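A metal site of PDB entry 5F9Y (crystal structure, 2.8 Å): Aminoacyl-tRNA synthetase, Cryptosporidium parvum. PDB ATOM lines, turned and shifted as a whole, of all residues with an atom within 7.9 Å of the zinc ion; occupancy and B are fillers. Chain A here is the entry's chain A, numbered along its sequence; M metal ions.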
ATOM      1  N   PRO A 442     -26.067  16.800  -0.870  1.00  0.00           N
ATOM      2  CA  PRO A 442     -27.353  16.769  -1.569  1.00  0.00           C
ATOM      3  C   PRO A 442     -27.325  15.748  -2.688  1.00  0.00           C
ATOM      4  O   PRO A 442     -26.338  15.622  -3.419  1.00  0.00           O
ATOM      5  CB  PRO A 442     -27.494  18.196  -2.102  1.00  0.00           C
ATOM      6  CG  PRO A 442     -26.086  18.694  -2.230  1.00  0.00           C
ATOM      7  CD  PRO A 442     -25.332  18.060  -1.101  1.00  0.00           C
ATOM      8  N   TRP A 443     -28.426  15.005  -2.823  1.00  0.00           N
ATOM      9  CA  TRP A 443     -28.470  13.870  -3.732  1.00  0.00           C
ATOM     10  C   TRP A 443     -29.881  13.727  -4.283  1.00  0.00           C
ATOM     11  O   TRP A 443     -30.858  14.040  -3.597  1.00  0.00           O
ATOM     12  CB  TRP A 443     -28.026  12.595  -3.018  1.00  0.00           C
ATOM     13  CG  TRP A 443     -27.889  11.401  -3.905  1.00  0.00           C
ATOM     14  CD1 TRP A 443     -27.385  11.367  -5.174  1.00  0.00           C
ATOM     15  CD2 TRP A 443     -28.256  10.057  -3.576  1.00  0.00           C
ATOM     16  NE1 TRP A 443     -27.431  10.082  -5.662  1.00  0.00           N
ATOM     17  CE2 TRP A 443     -27.961   9.264  -4.696  1.00  0.00           C
ATOM     18  CE3 TRP A 443     -28.822   9.453  -2.456  1.00  0.00           C
ATOM     19  CZ2 TRP A 443     -28.204   7.891  -4.721  1.00  0.00           C
ATOM     20  CZ3 TRP A 443     -29.055   8.089  -2.478  1.00  0.00           C
ATOM     21  CH2 TRP A 443     -28.750   7.322  -3.610  1.00  0.00           C
ATOM     22  N   CYS A 444     -29.976  13.241  -5.526  1.00  0.00           N
ATOM     23  CA  CYS A 444     -31.273  13.051  -6.172  1.00  0.00           C
ATOM     24  C   CYS A 444     -31.926  11.729  -5.812  1.00  0.00           C
ATOM     25  O   CYS A 444     -33.092  11.517  -6.169  1.00  0.00           O
ATOM     26  CB  CYS A 444     -31.106  13.143  -7.688  1.00  0.00           C
ATOM     27  SG  CYS A 444     -30.063  11.872  -8.418  1.00  0.00           S
ATOM     28  N   GLU A 445     -31.205  10.826  -5.135  1.00  0.00           N
ATOM     29  CA  GLU A 445     -31.719   9.527  -4.672  1.00  0.00           C
ATOM     30  C   GLU A 445     -32.126   8.598  -5.809  1.00  0.00           C
ATOM     31  O   GLU A 445     -32.915   7.676  -5.589  1.00  0.00           O
ATOM     32  CB  GLU A 445     -32.885   9.699  -3.689  1.00  0.00           C
ATOM     33  CG  GLU A 445     -32.599  10.638  -2.533  1.00  0.00           C
ATOM     34  CD  GLU A 445     -33.804  10.853  -1.658  1.00  0.00           C
ATOM     35  OE1 GLU A 445     -34.821  10.142  -1.828  1.00  0.00           O
ATOM     36  OE2 GLU A 445     -33.741  11.737  -0.780  1.00  0.00           O
ATOM     37  N   ASP A 446     -31.607   8.809  -7.009  1.00  0.00           N
ATOM     38  CA  ASP A 446     -31.901   7.926  -8.131  1.00  0.00           C
ATOM     39  C   ASP A 446     -30.948   6.737  -8.129  1.00  0.00           C
ATOM     40  O   ASP A 446     -29.800   6.840  -7.697  1.00  0.00           O
ATOM     41  CB  ASP A 446     -31.772   8.679  -9.462  1.00  0.00           C
ATOM     42  CG  ASP A 446     -32.854   9.726  -9.630  1.00  0.00           C
ATOM     43  OD1 ASP A 446     -33.898   9.631  -8.952  1.00  0.00           O
ATOM     44  OD2 ASP A 446     -32.662  10.652 -10.462  1.00  0.00           O
ATOM     45  N   SER A 448     -29.783   5.272 -10.803  1.00  0.00           N
ATOM     46  CA  SER A 448     -28.755   5.524 -11.811  1.00  0.00           C
ATOM     47  C   SER A 448     -27.618   6.369 -11.244  1.00  0.00           C
ATOM     48  O   SER A 448     -26.442   6.092 -11.499  1.00  0.00           O
ATOM     49  CB  SER A 448     -29.368   6.185 -13.033  1.00  0.00           C
ATOM     50  N   CYS A 449     -27.961   7.406 -10.472  1.00  0.00           N
ATOM     51  CA  CYS A 449     -26.935   8.264  -9.897  1.00  0.00           C
ATOM     52  C   CYS A 449     -26.068   7.511  -8.912  1.00  0.00           C
ATOM     53  O   CYS A 449     -24.860   7.727  -8.837  1.00  0.00           O
ATOM     54  CB  CYS A 449     -27.584   9.484  -9.239  1.00  0.00           C
ATOM     55  SG  CYS A 449     -26.434  10.797  -8.750  1.00  0.00           S
ATOM     56  N   GLU A 450     -26.671   6.597  -8.141  1.00  0.00           N
ATOM     57  CA  GLU A 450     -25.904   5.831  -7.165  1.00  0.00           C
ATOM     58  C   GLU A 450     -24.983   4.819  -7.836  1.00  0.00           C
ATOM     59  O   GLU A 450     -23.887   4.546  -7.339  1.00  0.00           O
ATOM     60  CB  GLU A 450     -26.842   5.120  -6.191  1.00  0.00           C
ATOM     61  CG  GLU A 450     -26.141   4.528  -4.975  1.00  0.00           C
ATOM     62  CD  GLU A 450     -27.114   3.975  -3.952  1.00  0.00           C
ATOM     63  OE1 GLU A 450     -26.664   3.559  -2.868  1.00  0.00           O
ATOM     64  OE2 GLU A 450     -28.340   3.957  -4.235  1.00  0.00           O
ATOM     65  N   ILE A 453     -21.956   6.670  -8.860  1.00  0.00           N
ATOM     66  CA  ILE A 453     -21.170   7.109  -7.710  1.00  0.00           C
ATOM     67  C   ILE A 453     -20.257   5.978  -7.233  1.00  0.00           C
ATOM     68  O   ILE A 453     -19.079   6.188  -6.963  1.00  0.00           O
ATOM     69  CB  ILE A 453     -22.094   7.594  -6.581  1.00  0.00           C
ATOM     70  CG1 ILE A 453     -22.692   8.964  -6.931  1.00  0.00           C
ATOM     71  CG2 ILE A 453     -21.342   7.667  -5.265  1.00  0.00           C
ATOM     72  CD1 ILE A 453     -23.853   9.368  -6.050  1.00  0.00           C
ATOM     73  N   LYS A 493     -28.636  21.643  -6.374  1.00  0.00           N
ATOM     74  CA  LYS A 493     -28.359  20.577  -7.321  1.00  0.00           C
ATOM     75  C   LYS A 493     -27.597  19.443  -6.645  1.00  0.00           C
ATOM     76  O   LYS A 493     -26.947  19.626  -5.607  1.00  0.00           O
ATOM     77  CB  LYS A 493     -27.559  21.094  -8.523  1.00  0.00           C
ATOM     78  N   CYS A 494     -27.710  18.259  -7.241  1.00  0.00           N
ATOM     79  CA  CYS A 494     -27.048  17.072  -6.720  1.00  0.00           C
ATOM     80  C   CYS A 494     -25.533  17.279  -6.682  1.00  0.00           C
ATOM     81  O   CYS A 494     -24.971  18.035  -7.466  1.00  0.00           O
ATOM     82  CB  CYS A 494     -27.399  15.866  -7.589  1.00  0.00           C
ATOM     83  SG  CYS A 494     -26.708  14.282  -7.051  1.00  0.00           S
ATOM     84  N   PHE A 495     -24.881  16.592  -5.733  1.00  0.00           N
ATOM     85  CA  PHE A 495     -23.426  16.634  -5.665  1.00  0.00           C
ATOM     86  C   PHE A 495     -22.768  15.817  -6.761  1.00  0.00           C
ATOM     87  O   PHE A 495     -21.533  15.878  -6.897  1.00  0.00           O
ATOM     88  CB  PHE A 495     -22.957  16.143  -4.296  1.00  0.00           C
ATOM     89  CG  PHE A 495     -22.819  14.644  -4.200  1.00  0.00           C
ATOM     90  CD1 PHE A 495     -21.566  14.058  -4.119  1.00  0.00           C
ATOM     91  CD2 PHE A 495     -23.944  13.833  -4.186  1.00  0.00           C
ATOM     92  CE1 PHE A 495     -21.438  12.682  -4.026  1.00  0.00           C
ATOM     93  CE2 PHE A 495     -23.816  12.456  -4.094  1.00  0.00           C
ATOM     94  CZ  PHE A 495     -22.566  11.877  -4.024  1.00  0.00           C
ATOM     95  N   PHE A 496     -23.535  15.073  -7.541  1.00  0.00           N
ATOM     96  CA  PHE A 496     -23.031  14.235  -8.612  1.00  0.00           C
ATOM     97  C   PHE A 496     -23.857  14.485  -9.868  1.00  0.00           C
ATOM     98  O   PHE A 496     -25.087  14.428  -9.814  1.00  0.00           O
ATOM     99  CB  PHE A 496     -23.067  12.754  -8.224  1.00  0.00           C
ATOM    100  CG  PHE A 496     -22.130  11.889  -9.015  1.00  0.00           C
ATOM    101  CD1 PHE A 496     -20.822  11.698  -8.588  1.00  0.00           C
ATOM    102  CD2 PHE A 496     -22.543  11.268 -10.184  1.00  0.00           C
ATOM    103  CE1 PHE A 496     -19.949  10.909  -9.304  1.00  0.00           C
ATOM    104  CE2 PHE A 496     -21.668  10.472 -10.912  1.00  0.00           C
ATOM    105  CZ  PHE A 496     -20.368  10.294 -10.468  1.00  0.00           C
ATOM    106  N   CYS A 497     -23.182  14.766 -10.974  1.00  0.00           N
ATOM    107  CA  CYS A 497     -23.827  15.075 -12.256  1.00  0.00           C
ATOM    108  C   CYS A 497     -24.732  16.286 -12.041  1.00  0.00           C
ATOM    109  O   CYS A 497     -24.279  17.270 -11.431  1.00  0.00           O
ATOM    110  CB  CYS A 497     -24.516  13.818 -12.790  1.00  0.00           C
ATOM    111  N   ASP A 498     -25.978  16.267 -12.502  1.00  0.00           N
ATOM    112  CA  ASP A 498     -26.868  17.411 -12.337  1.00  0.00           C
ATOM    113  C   ASP A 498     -28.307  16.916 -12.366  1.00  0.00           C
ATOM    114  O   ASP A 498     -28.771  16.394 -13.383  1.00  0.00           O
ATOM    115  CB  ASP A 498     -26.635  18.457 -13.434  1.00  0.00           C
ATOM    116  N   LYS A 499     -29.007  17.090 -11.252  1.00  0.00           N
ATOM    117  CA  LYS A 499     -30.426  16.737 -11.131  1.00  0.00           C
ATOM    118  C   LYS A 499     -30.958  17.387  -9.870  1.00  0.00           C
ATOM    119  O   LYS A 499     -30.205  17.668  -8.935  1.00  0.00           O
ATOM    120  CB  LYS A 499     -30.634  15.217 -11.090  1.00  0.00           C
ATOM    121  N   LEU A 500     -32.273  17.623  -9.846  1.00  0.00           N
ATOM    122  CA  LEU A 500     -32.921  18.243  -8.706  1.00  0.00           C
ATOM    123  C   LEU A 500     -32.775  17.386  -7.459  1.00  0.00           C
ATOM    124  O   LEU A 500     -33.382  16.319  -7.356  1.00  0.00           O
ATOM    125  CB  LEU A 500     -34.402  18.508  -9.008  1.00  0.00           C
ATOM    126  N   ALA A 501     -31.968  17.850  -6.499  1.00  0.00           N
ATOM    127  CA  ALA A 501     -31.728  17.079  -5.292  1.00  0.00           C
ATOM    128  C   ALA A 501     -32.952  17.090  -4.386  1.00  0.00           C
ATOM    129  O   ALA A 501     -33.600  18.124  -4.200  1.00  0.00           O
ATOM    130  CB  ALA A 501     -30.526  17.636  -4.539  1.00  0.00           C
HETATM  131 ZN    ZN M   1     -27.901  12.750  -8.917  1.00  0.00          ZN
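Merely in contact with the zinc ion: Phe 496 (3.4 Å). Four residues have an atom within 4 Å of the zinc ion: Cys 444, Cys 449, Cys 494 and Phe 496. The nearest printed residue that does not touch the zinc ion is Trp 443 (4.02 Å).
The zinc ion is bound by SG of Cys 444, at 2.4 Å. The side-chain sulfur (SG) of Cys 449 is bound to the zinc ion, 2.4 Å away. The side-chain sulfur (SG) of Cys 494 is bound to the zinc ion (2.7 Å).
The side-chain sulfur (SG) of Cys 444 sits close to the side-chain carboxylate (OD2) of Asp 446 (3.5 Å). NE1 of Trp 443 lies close to SG of Cys 449 (3.3 Å). The backbone carbonyl oxygen of Phe 496 lies close to the side-chain sulfur of Cys 494 (3.2 Å). The backbone carbonyl oxygen of Lys 499 lies within hydrogen-bond range of the backbone NH of Cys 494 (3.1 Å).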
